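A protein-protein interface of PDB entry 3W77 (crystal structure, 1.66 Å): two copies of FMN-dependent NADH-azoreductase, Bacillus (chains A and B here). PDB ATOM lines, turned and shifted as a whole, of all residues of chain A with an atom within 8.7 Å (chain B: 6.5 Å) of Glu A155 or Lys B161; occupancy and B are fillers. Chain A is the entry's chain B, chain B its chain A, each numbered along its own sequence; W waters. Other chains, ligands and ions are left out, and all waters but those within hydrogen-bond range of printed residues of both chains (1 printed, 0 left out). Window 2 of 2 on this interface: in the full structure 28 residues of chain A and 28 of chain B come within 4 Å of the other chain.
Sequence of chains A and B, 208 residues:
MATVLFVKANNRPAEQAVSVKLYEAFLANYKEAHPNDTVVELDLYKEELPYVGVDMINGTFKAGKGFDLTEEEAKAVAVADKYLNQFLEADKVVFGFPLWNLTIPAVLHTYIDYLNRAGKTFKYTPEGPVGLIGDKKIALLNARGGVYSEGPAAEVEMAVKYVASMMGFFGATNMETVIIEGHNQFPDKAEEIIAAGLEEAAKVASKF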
ATOM      1  N   LEU A 102      -7.527 -28.216 -12.860  1.00  0.00           N
ATOM      2  CA  LEU A 102      -6.702 -27.162 -12.213  1.00  0.00           C
ATOM      3  C   LEU A 102      -5.515 -26.642 -13.003  1.00  0.00           C
ATOM      4  O   LEU A 102      -4.906 -25.655 -12.568  1.00  0.00           O
ATOM      5  CB  LEU A 102      -6.214 -27.594 -10.810  1.00  0.00           C
ATOM      6  CG  LEU A 102      -7.285 -28.115  -9.832  1.00  0.00           C
ATOM      7  CD1 LEU A 102      -6.586 -28.608  -8.552  1.00  0.00           C
ATOM      8  CD2 LEU A 102      -8.337 -27.036  -9.552  1.00  0.00           C
ATOM      9  N   VAL A 147     -14.714 -19.529 -11.461  1.00  0.00           N
ATOM     10  CA  VAL A 147     -13.900 -18.317 -11.244  1.00  0.00           C
ATOM     11  C   VAL A 147     -12.681 -18.679 -10.390  1.00  0.00           C
ATOM     12  O   VAL A 147     -12.825 -19.351  -9.340  1.00  0.00           O
ATOM     13  CB  VAL A 147     -14.736 -17.198 -10.583  1.00  0.00           C
ATOM     14  CG1 VAL A 147     -13.852 -16.042 -10.108  1.00  0.00           C
ATOM     15  CG2 VAL A 147     -15.801 -16.718 -11.582  1.00  0.00           C
ATOM     16  N   TYR A 148     -11.487 -18.303 -10.866  1.00  0.00           N
ATOM     17  CA  TYR A 148     -10.231 -18.558 -10.130  1.00  0.00           C
ATOM     18  C   TYR A 148      -9.477 -17.300  -9.751  1.00  0.00           C
ATOM     19  O   TYR A 148      -8.423 -17.381  -9.094  1.00  0.00           O
ATOM     20  CB  TYR A 148      -9.298 -19.500 -10.911  1.00  0.00           C
ATOM     21  CG  TYR A 148      -9.778 -20.916 -10.906  1.00  0.00           C
ATOM     22  CD1 TYR A 148     -10.776 -21.345 -11.794  1.00  0.00           C
ATOM     23  CD2 TYR A 148      -9.230 -21.836 -10.021  1.00  0.00           C
ATOM     24  CE1 TYR A 148     -11.232 -22.661 -11.767  1.00  0.00           C
ATOM     25  CE2 TYR A 148      -9.648 -23.156 -10.017  1.00  0.00           C
ATOM     26  CZ  TYR A 148     -10.641 -23.569 -10.880  1.00  0.00           C
ATOM     27  OH  TYR A 148     -11.080 -24.886 -10.789  1.00  0.00           O
ATOM     28  N   SER A 149      -9.999 -16.129 -10.134  1.00  0.00           N
ATOM     29  CA  SER A 149      -9.334 -14.856  -9.762  1.00  0.00           C
ATOM     30  C   SER A 149      -9.665 -14.399  -8.334  1.00  0.00           C
ATOM     31  O   SER A 149      -9.012 -13.497  -7.796  1.00  0.00           O
ATOM     32  CB  SER A 149      -9.702 -13.765 -10.760  1.00  0.00           C
ATOM     33  OG  SER A 149     -11.086 -13.516 -10.742  1.00  0.00           O
ATOM     34  N   GLU A 150     -10.706 -14.992  -7.759  1.00  0.00           N
ATOM     35  CA  GLU A 150     -11.159 -14.703  -6.392  1.00  0.00           C
ATOM     36  C   GLU A 150     -11.944 -15.914  -5.898  1.00  0.00           C
ATOM     37  O   GLU A 150     -12.216 -16.846  -6.663  1.00  0.00           O
ATOM     38  CB  GLU A 150     -12.041 -13.437  -6.341  1.00  0.00           C
ATOM     39  CG  GLU A 150     -13.349 -13.535  -7.109  1.00  0.00           C
ATOM     40  CD  GLU A 150     -14.188 -12.264  -7.036  1.00  0.00           C
ATOM     41  OE1 GLU A 150     -15.202 -12.253  -6.331  1.00  0.00           O
ATOM     42  OE2 GLU A 150     -13.839 -11.266  -7.685  1.00  0.00           O
ATOM     43  N   GLY A 151     -12.322 -15.908  -4.629  1.00  0.00           N
ATOM     44  CA  GLY A 151     -13.117 -17.016  -4.114  1.00  0.00           C
ATOM     45  C   GLY A 151     -12.270 -18.198  -3.682  1.00  0.00           C
ATOM     46  O   GLY A 151     -11.057 -18.141  -3.747  1.00  0.00           O
ATOM     47  N   PRO A 152     -12.931 -19.269  -3.210  1.00  0.00           N
ATOM     48  CA  PRO A 152     -12.214 -20.408  -2.604  1.00  0.00           C
ATOM     49  C   PRO A 152     -11.327 -21.215  -3.548  1.00  0.00           C
ATOM     50  O   PRO A 152     -10.420 -21.901  -3.054  1.00  0.00           O
ATOM     51  CB  PRO A 152     -13.327 -21.281  -2.021  1.00  0.00           C
ATOM     52  CG  PRO A 152     -14.613 -20.754  -2.529  1.00  0.00           C
ATOM     53  CD  PRO A 152     -14.391 -19.352  -3.044  1.00  0.00           C
ATOM     54  N   ALA A 153     -11.551 -21.120  -4.863  1.00  0.00           N
ATOM     55  CA  ALA A 153     -10.727 -21.868  -5.844  1.00  0.00           C
ATOM     56  C   ALA A 153      -9.435 -21.129  -6.227  1.00  0.00           C
ATOM     57  O   ALA A 153      -8.518 -21.701  -6.825  1.00  0.00           O
ATOM     58  CB  ALA A 153     -11.544 -22.151  -7.094  1.00  0.00           C
ATOM     59  N   ALA A 154      -9.370 -19.837  -5.920  1.00  0.00           N
ATOM     60  CA  ALA A 154      -8.225 -19.026  -6.349  1.00  0.00           C
ATOM     61  C   ALA A 154      -6.881 -19.606  -5.931  1.00  0.00           C
ATOM     62  O   ALA A 154      -5.937 -19.582  -6.707  1.00  0.00           O
ATOM     63  CB  ALA A 154      -8.376 -17.584  -5.812  1.00  0.00           C
ATOM     64  N   GLU A 155      -6.814 -20.197  -4.742  1.00  0.00           N
ATOM     65  CA  GLU A 155      -5.557 -20.741  -4.235  1.00  0.00           C
ATOM     66  C   GLU A 155      -5.062 -21.994  -4.960  1.00  0.00           C
ATOM     67  O   GLU A 155      -3.907 -22.385  -4.753  1.00  0.00           O
ATOM     68  CB  GLU A 155      -5.654 -21.002  -2.719  1.00  0.00           C
ATOM     69  CG  GLU A 155      -6.626 -22.109  -2.325  1.00  0.00           C
ATOM     70  CD  GLU A 155      -6.582 -22.471  -0.838  1.00  0.00           C
ATOM     71  OE1 GLU A 155      -5.987 -21.718  -0.023  1.00  0.00           O
ATOM     72  OE2 GLU A 155      -7.145 -23.527  -0.474  1.00  0.00           O
ATOM     73  N   VAL A 156      -5.920 -22.619  -5.792  1.00  0.00           N
ATOM     74  CA  VAL A 156      -5.529 -23.838  -6.540  1.00  0.00           C
ATOM     75  C   VAL A 156      -5.482 -23.611  -8.059  1.00  0.00           C
ATOM     76  O   VAL A 156      -5.363 -24.577  -8.824  1.00  0.00           O
ATOM     77  CB  VAL A 156      -6.399 -25.091  -6.180  1.00  0.00           C
ATOM     78  CG1 VAL A 156      -6.152 -25.543  -4.734  1.00  0.00           C
ATOM     79  CG2 VAL A 156      -7.885 -24.832  -6.392  1.00  0.00           C
ATOM     80  N   GLU A 157      -5.518 -22.350  -8.507  1.00  0.00           N
ATOM     81  CA  GLU A 157      -5.327 -22.087  -9.952  1.00  0.00           C
ATOM     82  C   GLU A 157      -3.895 -22.430 -10.374  1.00  0.00           C
ATOM     83  O   GLU A 157      -2.923 -21.859  -9.846  1.00  0.00           O
ATOM     84  CB  GLU A 157      -5.622 -20.616 -10.280  1.00  0.00           C
ATOM     85  CG  GLU A 157      -5.952 -20.308 -11.753  1.00  0.00           C
ATOM     86  CD  GLU A 157      -4.786 -20.397 -12.740  1.00  0.00           C
ATOM     87  OE1 GLU A 157      -3.630 -20.062 -12.420  1.00  0.00           O
ATOM     88  OE2 GLU A 157      -5.065 -20.754 -13.901  1.00  0.00           O
ATOM     89  N   MET A 158      -3.736 -23.387 -11.299  1.00  0.00           N
ATOM     90  CA  MET A 158      -2.363 -23.840 -11.658  1.00  0.00           C
ATOM     91  C   MET A 158      -2.225 -23.981 -13.181  1.00  0.00           C
ATOM     92  O   MET A 158      -1.412 -24.765 -13.686  1.00  0.00           O
ATOM     93  CB  MET A 158      -2.014 -25.180 -10.954  1.00  0.00           C
ATOM     94  CG  MET A 158      -1.732 -24.967  -9.461  1.00  0.00           C
ATOM     95  SD  MET A 158      -1.400 -26.487  -8.547  1.00  0.00           S
ATOM     96  CE  MET A 158      -3.068 -26.941  -8.039  1.00  0.00           C
ATOM     97  N   LYS A 161      -1.134 -19.620 -13.871  1.00  0.00           N
ATOM     98  CA  LYS A 161      -0.008 -19.454 -12.935  1.00  0.00           C
ATOM     99  C   LYS A 161       1.203 -20.268 -13.369  1.00  0.00           C
ATOM    100  O   LYS A 161       2.356 -19.806 -13.238  1.00  0.00           O
ATOM    101  CB  LYS A 161      -0.438 -19.822 -11.512  1.00  0.00           C
ATOM    102  CG  LYS A 161       0.696 -19.756 -10.529  1.00  0.00           C
ATOM    103  CD  LYS A 161       0.165 -19.925  -9.140  1.00  0.00           C
ATOM    104  CE  LYS A 161       1.316 -20.272  -8.230  1.00  0.00           C
ATOM    105  NZ  LYS A 161       1.178 -19.509  -6.970  1.00  0.00           N
ATOM    106  N   PHE B  97       7.377 -39.251  -7.056  1.00  0.00           N
ATOM    107  CA  PHE B  97       7.624 -38.322  -8.163  1.00  0.00           C
ATOM    108  C   PHE B  97       8.595 -37.202  -7.799  1.00  0.00           C
ATOM    109  O   PHE B  97       8.633 -36.753  -6.654  1.00  0.00           O
ATOM    110  CB  PHE B  97       6.269 -37.679  -8.616  1.00  0.00           C
ATOM    111  CG  PHE B  97       5.475 -37.039  -7.492  1.00  0.00           C
ATOM    112  CD1 PHE B  97       4.624 -37.827  -6.696  1.00  0.00           C
ATOM    113  CD2 PHE B  97       5.569 -35.643  -7.211  1.00  0.00           C
ATOM    114  CE1 PHE B  97       3.886 -37.276  -5.647  1.00  0.00           C
ATOM    115  CE2 PHE B  97       4.819 -35.094  -6.162  1.00  0.00           C
ATOM    116  CZ  PHE B  97       3.981 -35.900  -5.368  1.00  0.00           C
ATOM    117  N   ARG B 144      12.768 -32.559  -4.313  1.00  0.00           N
ATOM    118  CA  ARG B 144      12.852 -31.294  -5.037  1.00  0.00           C
ATOM    119  C   ARG B 144      14.155 -30.606  -4.677  1.00  0.00           C
ATOM    120  O   ARG B 144      14.547 -30.584  -3.490  1.00  0.00           O
ATOM    121  CB  ARG B 144      11.623 -30.403  -4.775  1.00  0.00           C
ATOM    122  CG  ARG B 144      11.249 -30.195  -3.323  1.00  0.00           C
ATOM    123  CD  ARG B 144       9.803 -29.765  -3.185  1.00  0.00           C
ATOM    124  NE  ARG B 144       9.496 -29.324  -1.823  1.00  0.00           N
ATOM    125  CZ  ARG B 144       8.269 -29.266  -1.298  1.00  0.00           C
ATOM    126  NH1 ARG B 144       7.193 -29.673  -1.967  1.00  0.00           N
ATOM    127  NH2 ARG B 144       8.115 -28.835  -0.076  1.00  0.00           N
ATOM    128  N   GLU B 155       5.560 -20.081  -3.020  1.00  0.00           N
ATOM    129  CA  GLU B 155       4.368 -19.665  -3.770  1.00  0.00           C
ATOM    130  C   GLU B 155       4.162 -20.375  -5.110  1.00  0.00           C
ATOM    131  O   GLU B 155       3.052 -20.374  -5.658  1.00  0.00           O
ATOM    132  CB  GLU B 155       4.395 -18.147  -4.018  1.00  0.00           C
ATOM    133  CG  GLU B 155       5.787 -17.640  -4.438  1.00  0.00           C
ATOM    134  CD  GLU B 155       5.798 -16.404  -5.341  1.00  0.00           C
ATOM    135  OE1 GLU B 155       5.321 -15.308  -4.935  1.00  0.00           O
ATOM    136  OE2 GLU B 155       6.354 -16.517  -6.460  1.00  0.00           O
ATOM    137  N   GLU B 157       5.271 -23.705  -5.701  1.00  0.00           N
ATOM    138  CA  GLU B 157       5.294 -25.186  -5.654  1.00  0.00           C
ATOM    139  C   GLU B 157       3.997 -25.744  -6.261  1.00  0.00           C
ATOM    140  O   GLU B 157       2.889 -25.452  -5.772  1.00  0.00           O
ATOM    141  CB  GLU B 157       5.439 -25.700  -4.216  1.00  0.00           C
ATOM    142  CG  GLU B 157       6.049 -27.107  -4.117  1.00  0.00           C
ATOM    143  CD  GLU B 157       5.067 -28.252  -4.411  1.00  0.00           C
ATOM    144  OE1 GLU B 157       3.831 -28.141  -4.179  1.00  0.00           O
ATOM    145  OE2 GLU B 157       5.559 -29.331  -4.776  1.00  0.00           O
ATOM    146  N   MET B 158       4.124 -26.552  -7.321  1.00  0.00           N
ATOM    147  CA  MET B 158       2.935 -27.076  -8.017  1.00  0.00           C
ATOM    148  C   MET B 158       3.088 -28.573  -8.304  1.00  0.00           C
ATOM    149  O   MET B 158       2.517 -29.075  -9.276  1.00  0.00           O
ATOM    150  CB  MET B 158       2.663 -26.299  -9.318  1.00  0.00           C
ATOM    151  CG  MET B 158       2.218 -24.859  -9.026  1.00  0.00           C
ATOM    152  SD  MET B 158       1.877 -23.857 -10.496  1.00  0.00           S
ATOM    153  CE  MET B 158       3.472 -23.052 -10.647  1.00  0.00           C
ATOM    154  N   ALA B 159       3.857 -29.263  -7.453  1.00  0.00           N
ATOM    155  CA  ALA B 159       4.053 -30.707  -7.603  1.00  0.00           C
ATOM    156  C   ALA B 159       3.252 -31.426  -6.544  1.00  0.00           C
ATOM    157  O   ALA B 159       2.205 -31.977  -6.846  1.00  0.00           O
ATOM    158  CB  ALA B 159       5.553 -31.074  -7.544  1.00  0.00           C
ATOM    159  N   VAL B 160       3.727 -31.410  -5.300  1.00  0.00           N
ATOM    160  CA  VAL B 160       2.937 -31.939  -4.182  1.00  0.00           C
ATOM    161  C   VAL B 160       1.581 -31.256  -4.113  1.00  0.00           C
ATOM    162  O   VAL B 160       0.552 -31.925  -3.927  1.00  0.00           O
ATOM    163  CB  VAL B 160       3.697 -31.786  -2.842  1.00  0.00           C
ATOM    164  CG1 VAL B 160       2.822 -32.276  -1.699  1.00  0.00           C
ATOM    165  CG2 VAL B 160       4.961 -32.622  -2.916  1.00  0.00           C
ATOM    166  N   LYS B 161       1.562 -29.924  -4.273  1.00  0.00           N
ATOM    167  CA  LYS B 161       0.299 -29.203  -4.187  1.00  0.00           C
ATOM    168  C   LYS B 161      -0.698 -29.719  -5.236  1.00  0.00           C
ATOM    169  O   LYS B 161      -1.905 -29.790  -4.972  1.00  0.00           O
ATOM    170  CB  LYS B 161       0.504 -27.708  -4.376  1.00  0.00           C
ATOM    171  CG  LYS B 161      -0.811 -26.927  -4.327  1.00  0.00           C
ATOM    172  CD  LYS B 161      -0.578 -25.443  -4.237  1.00  0.00           C
ATOM    173  CE  LYS B 161      -1.901 -24.690  -4.111  1.00  0.00           C
ATOM    174  NZ  LYS B 161      -1.720 -23.322  -3.580  1.00  0.00           N
ATOM    175  N   TYR B 162      -0.195 -30.091  -6.417  1.00  0.00           N
ATOM    176  CA  TYR B 162      -1.091 -30.549  -7.481  1.00  0.00           C
ATOM    177  C   TYR B 162      -1.734 -31.916  -7.111  1.00  0.00           C
ATOM    178  O   TYR B 162      -2.966 -32.087  -7.147  1.00  0.00           O
ATOM    179  CB  TYR B 162      -0.370 -30.629  -8.859  1.00  0.00           C
ATOM    180  CG  TYR B 162      -1.372 -31.000  -9.910  1.00  0.00           C
ATOM    181  CD1 TYR B 162      -2.254 -30.021 -10.411  1.00  0.00           C
ATOM    182  CD2 TYR B 162      -1.514 -32.339 -10.350  1.00  0.00           C
ATOM    183  CE1 TYR B 162      -3.236 -30.363 -11.347  1.00  0.00           C
ATOM    184  CE2 TYR B 162      -2.507 -32.687 -11.289  1.00  0.00           C
ATOM    185  CZ  TYR B 162      -3.353 -31.699 -11.773  1.00  0.00           C
ATOM    186  OH  TYR B 162      -4.358 -32.010 -12.662  1.00  0.00           O
ATOM    187  N   VAL B 163      -0.889 -32.883  -6.784  1.00  0.00           N
ATOM    188  CA  VAL B 163      -1.352 -34.248  -6.490  1.00  0.00           C
ATOM    189  C   VAL B 163      -2.235 -34.225  -5.245  1.00  0.00           C
ATOM    190  O   VAL B 163      -3.303 -34.853  -5.227  1.00  0.00           O
ATOM    191  CB  VAL B 163      -0.164 -35.223  -6.277  1.00  0.00           C
ATOM    192  CG1 VAL B 163      -0.725 -36.653  -6.166  1.00  0.00           C
ATOM    193  CG2 VAL B 163       0.809 -35.173  -7.452  1.00  0.00           C
ATOM    194  N   ALA B 164      -1.836 -33.463  -4.233  1.00  0.00           N
ATOM    195  CA  ALA B 164      -2.640 -33.403  -3.006  1.00  0.00           C
ATOM    196  C   ALA B 164      -4.018 -32.782  -3.257  1.00  0.00           C
ATOM    197  O   ALA B 164      -5.026 -33.235  -2.672  1.00  0.00           O
ATOM    198  CB  ALA B 164      -1.898 -32.659  -1.909  1.00  0.00           C
ATOM    199  N   SER B 165      -4.068 -31.765  -4.114  1.00  0.00           N
ATOM    200  CA  SER B 165      -5.335 -31.101  -4.470  1.00  0.00           C
ATOM    201  C   SER B 165      -6.289 -32.034  -5.216  1.00  0.00           C
ATOM    202  O   SER B 165      -7.484 -32.071  -4.892  1.00  0.00           O
ATOM    203  CB  SER B 165      -5.103 -29.835  -5.314  1.00  0.00           C
ATOM    204  OG  SER B 165      -4.402 -28.844  -4.546  1.00  0.00           O
ATOM    205  N   MET B 166      -5.757 -32.797  -6.186  1.00  0.00           N
ATOM    206  CA  MET B 166      -6.594 -33.718  -6.961  1.00  0.00           C
ATOM    207  C   MET B 166      -7.017 -34.903  -6.092  1.00  0.00           C
ATOM    208  O   MET B 166      -8.176 -35.266  -6.105  1.00  0.00           O
ATOM    209  CB  MET B 166      -5.933 -34.187  -8.281  1.00  0.00           C
ATOM    210  CG  MET B 166      -5.779 -33.062  -9.329  1.00  0.00           C
ATOM    211  SD  MET B 166      -7.332 -32.157  -9.685  1.00  0.00           S
ATOM    212  CE  MET B 166      -8.363 -33.498 -10.225  1.00  0.00           C
HETATM  213  O   HOH W   1       0.918 -22.790  -5.858  1.00  0.00           O
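Hydrophobic or aromatic side chains of chain B that line the printed part of chain A: Met B158, Tyr B162 and Met B166.
Hydrophobic or aromatic side chains of chain A within 4 Å of the printed part of chain B: Leu A102, Val A156 and Met A158.
Glu A155 touches Lys B161, and with the chains exchanged Lys A161 touches Glu B155.
Met B158 touches its own counterpart, Met A158.
Positions printed for both chains: 155, 157, 158 and 161.
The backbone carbonyl oxygen of Glu B155 lies within hydrogen-bond range of the side-chain amino group of Lys A161, at 2.4 Å.
NZ of Lys B161 sits at hydrogen-bond distance from O of Glu A155 (2.7 Å).
The side-chain carboxylate (OE1) of Glu B157 sits at hydrogen-bond distance from the backbone NH (N) of Lys B161 (2.9 Å).
OG of Ser B165 is in hydrogen-bond range of O of Lys B161 (2.7 Å).
O of Leu A102 lies within hydrogen-bond range of N of Met A158.
N of Lys A161 is in hydrogen-bond range of OE1 of Glu A157.
Glu A155 touches one residue of chain B.
No residue of chain A comes within 4 Å of Val B160.
Of the printed residues of chain A, Tyr B162 touches Met A158.
Of the printed residues of chain B, Met A158 touches Met B158 and Tyr B162.
Of the printed residues of chain B, Leu A102 touches Ser B165 (3.8 Å) and Met B166 (3.8 Å).
Printed residues of chain A within 4 Å of Met B158: Met A158.
Ala A154 touches none of the printed residues of chain B.
The nearest residue of chain A that does not touch Lys B161 is Met A158 (4.3 Å).
The nearest printed residue of chain A that does not touch Tyr B162 is Leu A102 (4.1 Å).
Among the printed residues, merely in contact across the chains: Val A156 with Ser B165 (3.7 Å), Leu A102 with Ser B165 (3.8 Å), Leu A102 with Met B166 (3.8 Å), Met A158 with Met B158 (3.9 Å) and Met A158 with Tyr B162 (3.97 Å).
Water W1 lies within hydrogen-bond range of O of Glu B155 (3.2 Å), O of Glu B157 (3.3 Å) and NZ of Lys A161 (3.5 Å).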
